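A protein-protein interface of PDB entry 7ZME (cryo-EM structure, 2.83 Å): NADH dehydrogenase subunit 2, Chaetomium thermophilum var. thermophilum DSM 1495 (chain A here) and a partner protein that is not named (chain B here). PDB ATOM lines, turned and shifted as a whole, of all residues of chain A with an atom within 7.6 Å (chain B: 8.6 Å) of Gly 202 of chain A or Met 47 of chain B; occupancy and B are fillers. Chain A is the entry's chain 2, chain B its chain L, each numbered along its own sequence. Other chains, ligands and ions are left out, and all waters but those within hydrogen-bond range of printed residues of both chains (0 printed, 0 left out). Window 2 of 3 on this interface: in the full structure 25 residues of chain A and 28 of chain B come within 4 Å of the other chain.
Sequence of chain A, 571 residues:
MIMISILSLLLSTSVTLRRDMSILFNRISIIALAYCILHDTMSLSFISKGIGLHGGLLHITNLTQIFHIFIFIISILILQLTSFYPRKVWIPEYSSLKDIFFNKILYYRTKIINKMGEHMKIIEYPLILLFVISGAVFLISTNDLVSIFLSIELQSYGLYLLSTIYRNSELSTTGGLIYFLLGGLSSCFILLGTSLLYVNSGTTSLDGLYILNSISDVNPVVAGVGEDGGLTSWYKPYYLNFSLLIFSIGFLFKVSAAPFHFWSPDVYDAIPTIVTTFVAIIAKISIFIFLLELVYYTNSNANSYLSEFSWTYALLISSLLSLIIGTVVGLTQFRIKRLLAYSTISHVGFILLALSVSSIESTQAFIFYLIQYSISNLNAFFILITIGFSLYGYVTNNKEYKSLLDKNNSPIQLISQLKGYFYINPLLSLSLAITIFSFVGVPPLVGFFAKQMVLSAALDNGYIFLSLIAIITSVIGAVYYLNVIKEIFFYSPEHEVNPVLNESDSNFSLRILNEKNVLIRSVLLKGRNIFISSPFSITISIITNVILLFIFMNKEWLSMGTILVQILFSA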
ATOM      1  N   SER A 195       3.717 -15.404 -27.349  1.00  0.00           N
ATOM      2  CA  SER A 195       2.642 -14.455 -27.092  1.00  0.00           C
ATOM      3  C   SER A 195       1.437 -15.145 -26.474  1.00  0.00           C
ATOM      4  O   SER A 195       0.839 -14.631 -25.524  1.00  0.00           O
ATOM      5  CB  SER A 195       2.247 -13.742 -28.386  1.00  0.00           C
ATOM      6  OG  SER A 195       1.437 -14.566 -29.201  1.00  0.00           O
ATOM      7  N   LEU A 196       1.074 -16.319 -26.982  1.00  0.00           N
ATOM      8  CA  LEU A 196      -0.077 -17.023 -26.433  1.00  0.00           C
ATOM      9  C   LEU A 196       0.183 -17.503 -25.015  1.00  0.00           C
ATOM     10  O   LEU A 196      -0.754 -17.620 -24.221  1.00  0.00           O
ATOM     11  CB  LEU A 196      -0.451 -18.191 -27.337  1.00  0.00           C
ATOM     12  CG  LEU A 196      -1.002 -17.716 -28.677  1.00  0.00           C
ATOM     13  CD1 LEU A 196      -1.062 -18.857 -29.661  1.00  0.00           C
ATOM     14  CD2 LEU A 196      -2.358 -17.059 -28.496  1.00  0.00           C
ATOM     15  N   LEU A 197       1.441 -17.787 -24.682  1.00  0.00           N
ATOM     16  CA  LEU A 197       1.779 -18.151 -23.311  1.00  0.00           C
ATOM     17  C   LEU A 197       1.572 -16.976 -22.367  1.00  0.00           C
ATOM     18  O   LEU A 197       0.962 -17.123 -21.302  1.00  0.00           O
ATOM     19  CB  LEU A 197       3.222 -18.648 -23.250  1.00  0.00           C
ATOM     20  CG  LEU A 197       3.441 -20.110 -23.632  1.00  0.00           C
ATOM     21  CD1 LEU A 197       4.875 -20.501 -23.387  1.00  0.00           C
ATOM     22  CD2 LEU A 197       2.495 -21.019 -22.861  1.00  0.00           C
ATOM     23  N   TYR A 198       2.070 -15.795 -22.747  1.00  0.00           N
ATOM     24  CA  TYR A 198       1.924 -14.611 -21.906  1.00  0.00           C
ATOM     25  C   TYR A 198       0.475 -14.151 -21.842  1.00  0.00           C
ATOM     26  O   TYR A 198      -0.005 -13.736 -20.782  1.00  0.00           O
ATOM     27  CB  TYR A 198       2.827 -13.491 -22.425  1.00  0.00           C
ATOM     28  CG  TYR A 198       2.473 -12.115 -21.910  1.00  0.00           C
ATOM     29  CD1 TYR A 198       2.846 -11.711 -20.639  1.00  0.00           C
ATOM     30  CD2 TYR A 198       1.767 -11.221 -22.701  1.00  0.00           C
ATOM     31  CE1 TYR A 198       2.523 -10.462 -20.167  1.00  0.00           C
ATOM     32  CE2 TYR A 198       1.437  -9.969 -22.239  1.00  0.00           C
ATOM     33  CZ  TYR A 198       1.819  -9.594 -20.972  1.00  0.00           C
ATOM     34  OH  TYR A 198       1.491  -8.347 -20.513  1.00  0.00           O
ATOM     35  N   VAL A 199      -0.233 -14.214 -22.966  1.00  0.00           N
ATOM     36  CA  VAL A 199      -1.615 -13.751 -23.024  1.00  0.00           C
ATOM     37  C   VAL A 199      -2.522 -14.591 -22.136  1.00  0.00           C
ATOM     38  O   VAL A 199      -3.489 -14.079 -21.559  1.00  0.00           O
ATOM     39  CB  VAL A 199      -2.079 -13.731 -24.496  1.00  0.00           C
ATOM     40  CG1 VAL A 199      -3.550 -13.568 -24.594  1.00  0.00           C
ATOM     41  CG2 VAL A 199      -1.423 -12.571 -25.220  1.00  0.00           C
ATOM     42  N   ASN A 200      -2.219 -15.873 -21.982  1.00  0.00           N
ATOM     43  CA  ASN A 200      -3.097 -16.757 -21.229  1.00  0.00           C
ATOM     44  C   ASN A 200      -2.667 -16.940 -19.784  1.00  0.00           C
ATOM     45  O   ASN A 200      -3.509 -17.228 -18.930  1.00  0.00           O
ATOM     46  CB  ASN A 200      -3.172 -18.119 -21.916  1.00  0.00           C
ATOM     47  CG  ASN A 200      -4.329 -18.223 -22.879  1.00  0.00           C
ATOM     48  OD1 ASN A 200      -5.454 -18.497 -22.477  1.00  0.00           O
ATOM     49  ND2 ASN A 200      -4.060 -18.009 -24.157  1.00  0.00           N
ATOM     50  N   SER A 201      -1.381 -16.775 -19.486  1.00  0.00           N
ATOM     51  CA  SER A 201      -0.864 -16.973 -18.141  1.00  0.00           C
ATOM     52  C   SER A 201      -0.550 -15.673 -17.417  1.00  0.00           C
ATOM     53  O   SER A 201      -0.272 -15.710 -16.215  1.00  0.00           O
ATOM     54  CB  SER A 201       0.396 -17.838 -18.185  1.00  0.00           C
ATOM     55  OG  SER A 201       1.323 -17.321 -19.119  1.00  0.00           O
ATOM     56  N   GLY A 202      -0.577 -14.537 -18.109  1.00  0.00           N
ATOM     57  CA  GLY A 202      -0.253 -13.267 -17.497  1.00  0.00           C
ATOM     58  C   GLY A 202       1.197 -13.077 -17.114  1.00  0.00           C
ATOM     59  O   GLY A 202       1.569 -11.974 -16.705  1.00  0.00           O
ATOM     60  N   THR A 203       2.030 -14.106 -17.239  1.00  0.00           N
ATOM     61  CA  THR A 203       3.429 -14.049 -16.855  1.00  0.00           C
ATOM     62  C   THR A 203       4.308 -14.232 -18.081  1.00  0.00           C
ATOM     63  O   THR A 203       3.896 -14.805 -19.092  1.00  0.00           O
ATOM     64  CB  THR A 203       3.773 -15.117 -15.797  1.00  0.00           C
ATOM     65  OG1 THR A 203       5.170 -15.060 -15.488  1.00  0.00           O
ATOM     66  CG2 THR A 203       3.438 -16.509 -16.292  1.00  0.00           C
ATOM     67  N   THR A 204       5.535 -13.726 -17.979  1.00  0.00           N
ATOM     68  CA  THR A 204       6.524 -13.854 -19.034  1.00  0.00           C
ATOM     69  C   THR A 204       7.727 -14.695 -18.640  1.00  0.00           C
ATOM     70  O   THR A 204       8.565 -14.980 -19.497  1.00  0.00           O
ATOM     71  CB  THR A 204       6.994 -12.466 -19.493  1.00  0.00           C
ATOM     72  OG1 THR A 204       7.843 -12.596 -20.638  1.00  0.00           O
ATOM     73  CG2 THR A 204       7.723 -11.742 -18.381  1.00  0.00           C
ATOM     74  N   SER A 205       7.829 -15.110 -17.385  1.00  0.00           N
ATOM     75  CA  SER A 205       8.915 -15.968 -16.944  1.00  0.00           C
ATOM     76  C   SER A 205       8.532 -17.434 -17.093  1.00  0.00           C
ATOM     77  O   SER A 205       7.418 -17.841 -16.758  1.00  0.00           O
ATOM     78  CB  SER A 205       9.279 -15.677 -15.490  1.00  0.00           C
ATOM     79  OG  SER A 205       8.295 -16.184 -14.610  1.00  0.00           O
ATOM     80  N   LEU A 209       5.710 -20.078 -15.517  1.00  0.00           N
ATOM     81  CA  LEU A 209       4.966 -21.011 -16.358  1.00  0.00           C
ATOM     82  C   LEU A 209       5.109 -22.443 -15.865  1.00  0.00           C
ATOM     83  O   LEU A 209       4.161 -23.231 -15.948  1.00  0.00           O
ATOM     84  CB  LEU A 209       5.433 -20.902 -17.809  1.00  0.00           C
ATOM     85  CG  LEU A 209       5.041 -19.644 -18.582  1.00  0.00           C
ATOM     86  CD1 LEU A 209       5.785 -19.564 -19.901  1.00  0.00           C
ATOM     87  CD2 LEU A 209       3.548 -19.653 -18.822  1.00  0.00           C
ATOM     88  N   LEU A 212       2.730 -22.994 -12.821  1.00  0.00           N
ATOM     89  CA  LEU A 212       1.315 -23.138 -13.262  1.00  0.00           C
ATOM     90  C   LEU A 212       1.093 -24.541 -13.846  1.00  0.00           C
ATOM     91  O   LEU A 212       0.051 -25.125 -13.550  1.00  0.00           O
ATOM     92  CB  LEU A 212       0.977 -22.037 -14.270  1.00  0.00           C
ATOM     93  CG  LEU A 212       0.960 -20.609 -13.730  1.00  0.00           C
ATOM     94  CD1 LEU A 212       0.963 -19.606 -14.870  1.00  0.00           C
ATOM     95  CD2 LEU A 212      -0.239 -20.382 -12.827  1.00  0.00           C
ATOM     96  N   TYR A 239      -3.903 -24.172 -22.910  1.00  0.00           N
ATOM     97  CA  TYR A 239      -3.080 -23.287 -23.722  1.00  0.00           C
ATOM     98  C   TYR A 239      -1.606 -23.647 -23.652  1.00  0.00           C
ATOM     99  O   TYR A 239      -0.874 -23.413 -24.616  1.00  0.00           O
ATOM    100  CB  TYR A 239      -3.286 -21.838 -23.286  1.00  0.00           C
ATOM    101  CG  TYR A 239      -2.764 -21.528 -21.902  1.00  0.00           C
ATOM    102  CD1 TYR A 239      -3.542 -21.756 -20.780  1.00  0.00           C
ATOM    103  CD2 TYR A 239      -1.490 -21.004 -21.719  1.00  0.00           C
ATOM    104  CE1 TYR A 239      -3.070 -21.472 -19.522  1.00  0.00           C
ATOM    105  CE2 TYR A 239      -1.012 -20.716 -20.462  1.00  0.00           C
ATOM    106  CZ  TYR A 239      -1.806 -20.953 -19.368  1.00  0.00           C
ATOM    107  OH  TYR A 239      -1.337 -20.675 -18.109  1.00  0.00           O
ATOM    108  N   LEU B  39      -2.058  -8.364 -30.512  1.00  0.00           N
ATOM    109  CA  LEU B  39      -2.671  -9.234 -29.513  1.00  0.00           C
ATOM    110  C   LEU B  39      -2.051  -9.021 -28.140  1.00  0.00           C
ATOM    111  O   LEU B  39      -2.760  -9.000 -27.127  1.00  0.00           O
ATOM    112  CB  LEU B  39      -2.541 -10.696 -29.935  1.00  0.00           C
ATOM    113  CG  LEU B  39      -2.967 -11.711 -28.875  1.00  0.00           C
ATOM    114  CD1 LEU B  39      -4.470 -11.721 -28.718  1.00  0.00           C
ATOM    115  CD2 LEU B  39      -2.445 -13.094 -29.204  1.00  0.00           C
ATOM    116  N   ILE B  40      -0.727  -8.866 -28.086  1.00  0.00           N
ATOM    117  CA  ILE B  40      -0.043  -8.645 -26.817  1.00  0.00           C
ATOM    118  C   ILE B  40      -0.450  -7.306 -26.216  1.00  0.00           C
ATOM    119  O   ILE B  40      -0.592  -7.174 -24.996  1.00  0.00           O
ATOM    120  CB  ILE B  40       1.480  -8.745 -27.016  1.00  0.00           C
ATOM    121  CG1 ILE B  40       1.848 -10.121 -27.572  1.00  0.00           C
ATOM    122  CG2 ILE B  40       2.222  -8.496 -25.721  1.00  0.00           C
ATOM    123  CD1 ILE B  40       3.248 -10.203 -28.120  1.00  0.00           C
ATOM    124  N   LEU B  41      -0.703  -6.301 -27.035  1.00  0.00           N
ATOM    125  CA  LEU B  41      -1.082  -4.950 -26.537  1.00  0.00           C
ATOM    126  C   LEU B  41      -2.467  -4.972 -25.905  1.00  0.00           C
ATOM    127  O   LEU B  41      -2.622  -4.392 -24.824  1.00  0.00           O
ATOM    128  CB  LEU B  41      -0.951  -3.899 -27.638  1.00  0.00           C
ATOM    129  CG  LEU B  41       0.488  -3.491 -27.949  1.00  0.00           C
ATOM    130  CD1 LEU B  41       0.568  -2.648 -29.208  1.00  0.00           C
ATOM    131  CD2 LEU B  41       1.110  -2.760 -26.774  1.00  0.00           C
ATOM    132  N   LEU B  42      -3.443  -5.554 -26.586  1.00  0.00           N
ATOM    133  CA  LEU B  42      -4.825  -5.631 -26.049  1.00  0.00           C
ATOM    134  C   LEU B  42      -4.855  -6.443 -24.752  1.00  0.00           C
ATOM    135  O   LEU B  42      -5.586  -6.044 -23.852  1.00  0.00           O
ATOM    136  CB  LEU B  42      -5.718  -6.233 -27.136  1.00  0.00           C
ATOM    137  CG  LEU B  42      -5.790  -5.448 -28.442  1.00  0.00           C
ATOM    138  CD1 LEU B  42      -6.662  -6.167 -29.454  1.00  0.00           C
ATOM    139  CD2 LEU B  42      -6.313  -4.049 -28.197  1.00  0.00           C
ATOM    140  N   SER B  43      -4.114  -7.545 -24.670  1.00  0.00           N
ATOM    141  CA  SER B  43      -4.034  -8.392 -23.453  1.00  0.00           C
ATOM    142  C   SER B  43      -3.407  -7.623 -22.304  1.00  0.00           C
ATOM    143  O   SER B  43      -3.886  -7.742 -21.177  1.00  0.00           O
ATOM    144  CB  SER B  43      -3.244  -9.614 -23.750  1.00  0.00           C
ATOM    145  OG  SER B  43      -3.781 -10.273 -24.883  1.00  0.00           O
ATOM    146  N   SER B  44      -2.319  -6.912 -22.586  1.00  0.00           N
ATOM    147  CA  SER B  44      -1.643  -6.064 -21.574  1.00  0.00           C
ATOM    148  C   SER B  44      -2.659  -5.112 -20.938  1.00  0.00           C
ATOM    149  O   SER B  44      -2.603  -4.939 -19.712  1.00  0.00           O
ATOM    150  CB  SER B  44      -0.513  -5.326 -22.207  1.00  0.00           C
ATOM    151  OG  SER B  44       0.307  -6.220 -22.923  1.00  0.00           O
ATOM    152  N   LEU B  45      -3.473  -4.447 -21.755  1.00  0.00           N
ATOM    153  CA  LEU B  45      -4.495  -3.504 -21.245  1.00  0.00           C
ATOM    154  C   LEU B  45      -5.494  -4.235 -20.350  1.00  0.00           C
ATOM    155  O   LEU B  45      -5.896  -3.647 -19.342  1.00  0.00           O
ATOM    156  CB  LEU B  45      -5.181  -2.850 -22.445  1.00  0.00           C
ATOM    157  CG  LEU B  45      -6.251  -1.806 -22.141  1.00  0.00           C
ATOM    158  CD1 LEU B  45      -5.660  -0.628 -21.385  1.00  0.00           C
ATOM    159  CD2 LEU B  45      -6.908  -1.336 -23.425  1.00  0.00           C
ATOM    160  N   ASN B  46      -5.859  -5.469 -20.685  1.00  0.00           N
ATOM    161  CA  ASN B  46      -6.905  -6.185 -19.914  1.00  0.00           C
ATOM    162  C   ASN B  46      -6.307  -6.760 -18.630  1.00  0.00           C
ATOM    163  O   ASN B  46      -7.083  -7.001 -17.707  1.00  0.00           O
ATOM    164  CB  ASN B  46      -7.469  -7.368 -20.698  1.00  0.00           C
ATOM    165  CG  ASN B  46      -8.008  -7.020 -22.067  1.00  0.00           C
ATOM    166  OD1 ASN B  46      -7.992  -7.853 -22.969  1.00  0.00           O
ATOM    167  ND2 ASN B  46      -8.477  -5.798 -22.240  1.00  0.00           N
ATOM    168  N   MET B  47      -4.982  -6.947 -18.570  1.00  0.00           N
ATOM    169  CA  MET B  47      -4.326  -7.456 -17.340  1.00  0.00           C
ATOM    170  C   MET B  47      -3.527  -6.380 -16.596  1.00  0.00           C
ATOM    171  O   MET B  47      -2.848  -6.754 -15.635  1.00  0.00           O
ATOM    172  CB  MET B  47      -3.420  -8.635 -17.692  1.00  0.00           C
ATOM    173  CG  MET B  47      -4.109  -9.684 -18.547  1.00  0.00           C
ATOM    174  SD  MET B  47      -3.059 -11.080 -19.022  1.00  0.00           S
ATOM    175  CE  MET B  47      -1.834 -10.280 -20.057  1.00  0.00           C
ATOM    176  N   ASP B  48      -3.627  -5.107 -16.987  1.00  0.00           N
ATOM    177  CA  ASP B  48      -2.905  -3.981 -16.320  1.00  0.00           C
ATOM    178  C   ASP B  48      -1.395  -4.234 -16.312  1.00  0.00           C
ATOM    179  O   ASP B  48      -0.784  -4.067 -15.268  1.00  0.00           O
ATOM    180  CB  ASP B  48      -3.459  -3.731 -14.919  1.00  0.00           C
ATOM    181  CG  ASP B  48      -3.314  -2.300 -14.461  1.00  0.00           C
ATOM    182  OD1 ASP B  48      -3.695  -1.410 -15.240  1.00  0.00           O
ATOM    183  OD2 ASP B  48      -2.816  -2.096 -13.337  1.00  0.00           O
ATOM    184  N   ASP B  49      -0.827  -4.654 -17.436  1.00  0.00           N
ATOM    185  CA  ASP B  49       0.603  -5.042 -17.491  1.00  0.00           C
ATOM    186  C   ASP B  49       1.411  -4.110 -18.388  1.00  0.00           C
ATOM    187  O   ASP B  49       1.166  -4.109 -19.600  1.00  0.00           O
ATOM    188  CB  ASP B  49       0.716  -6.379 -18.201  1.00  0.00           C
ATOM    189  CG  ASP B  49       0.581  -7.586 -17.304  1.00  0.00           C
ATOM    190  OD1 ASP B  49       1.151  -7.563 -16.201  1.00  0.00           O
ATOM    191  OD2 ASP B  49      -0.076  -8.540 -17.738  1.00  0.00           O
ATOM    192  N   ILE B  50       2.362  -3.382 -17.830  1.00  0.00           N
ATOM    193  CA  ILE B  50       3.238  -2.539 -18.626  1.00  0.00           C
ATOM    194  C   ILE B  50       4.324  -3.364 -19.301  1.00  0.00           C
ATOM    195  O   ILE B  50       5.035  -2.856 -20.175  1.00  0.00           O
ATOM    196  CB  ILE B  50       3.809  -1.410 -17.741  1.00  0.00           C
ATOM    197  CG1 ILE B  50       4.248  -0.228 -18.601  1.00  0.00           C
ATOM    198  CG2 ILE B  50       4.959  -1.910 -16.899  1.00  0.00           C
ATOM    199  CD1 ILE B  50       3.105   0.453 -19.307  1.00  0.00           C
ATOM    200  N   ILE B  51       4.441  -4.640 -18.930  1.00  0.00           N
ATOM    201  CA  ILE B  51       5.446  -5.518 -19.521  1.00  0.00           C
ATOM    202  C   ILE B  51       5.066  -5.899 -20.943  1.00  0.00           C
ATOM    203  O   ILE B  51       5.929  -6.022 -21.818  1.00  0.00           O
ATOM    204  CB  ILE B  51       5.653  -6.752 -18.626  1.00  0.00           C
ATOM    205  CG1 ILE B  51       6.326  -6.321 -17.334  1.00  0.00           C
ATOM    206  CG2 ILE B  51       6.477  -7.821 -19.321  1.00  0.00           C
ATOM    207  CD1 ILE B  51       7.580  -5.580 -17.571  1.00  0.00           C
ATOM    208  N   GLY B  52       3.774  -6.092 -21.203  1.00  0.00           N
ATOM    209  CA  GLY B  52       3.354  -6.416 -22.550  1.00  0.00           C
ATOM    210  C   GLY B  52       3.474  -5.267 -23.523  1.00  0.00           C
ATOM    211  O   GLY B  52       3.584  -5.501 -24.729  1.00  0.00           O
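The side-chain hydroxyl of Ser 44 of chain B sits at hydrogen-bond distance from the backbone carbonyl oxygen of Ile 40 of chain B. The backbone carbonyl oxygen of Leu 39 of chain B is in hydrogen-bond range of the side-chain hydroxyl of Ser 43 of chain B, 2.8 Å away. The backbone NH of Asp 49 of chain B sits at hydrogen-bond distance from the backbone carbonyl oxygen of Ser 44 of chain B (2.9 Å).
The side-chain hydroxyl of Tyr 198 of chain A lies close to the side-chain carboxylate of Asp 49 of chain B, 3.2 Å away. N of Gly 52 of chain B sits at hydrogen-bond distance from OH of Tyr 198 of chain A, at 3.3 Å. The side-chain hydroxyl (OH) of Tyr 198 of chain A sits at hydrogen-bond distance from the side-chain hydroxyl (OG) of Ser 44 of chain B (3.4 Å).
Of the 14 printed residues of chain B, 6 touch a printed residue of chain A. Printed residues of chain B that touch a printed residue of chain A: Ile 40, Ser 43, Ser 44, Met 47, Asp 49 and Gly 52. Hydrophobic or aromatic side chains of chain B that line the printed part of chain A: Ile 40 and Met 47. Hydrophobic or aromatic side chains of chain A that line the printed part of chain B: Tyr 198 and Val 199.
Ile 40 of chain B touches Ser 195 of chain A. Tyr 198 of chain A touches Ile 40 of chain B (CE2 to CG2, 3.9 Å). Tyr 198 of chain A touches Met 47 of chain B (CZ to CE, 3.8 Å). CG2 of Val 199 of chain A touches OG of Ser 43 of chain B, at 3.3 Å. Met 47 of chain B touches Val 199 of chain A (SD to O, 3.95 Å). Met 47 of chain B touches Gly 202 of chain A (SD to CA, 3.9 Å). Asp 49 of chain B touches Gly 202 of chain A.
Of the printed residues of chain B, Ser 195 of chain A touches Ile 40 (3.7 Å). Printed residues of chain B within 4 Å of Tyr 198 of chain A: Ile 40 (3.9 Å), Ser 44 (3.4 Å), Met 47 (3.8 Å), Asp 49 (3.1 Å) and Gly 52 (3.3 Å). Printed residues of chain B within 4 Å of Val 199 of chain A: Ser 43 and Met 47. No residue of chain B comes within 4 Å of Ser 201 of chain A. Leu 212 of chain A touches none of the printed residues of chain B. Printed residues of chain A within 4 Å of Ile 40 of chain B: Ser 195 and Tyr 198. Printed residues of chain A within 4 Å of Ser 43 of chain B: Val 199. Of the printed residues of chain A, Met 47 of chain B touches Tyr 198, Val 199 and Gly 202. Ile 50 of chain B touches none of the printed residues of chain A. The nearest printed residue of chain A that does not touch Ser 43 of chain B is Tyr 198 of chain A (4.9 Å).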
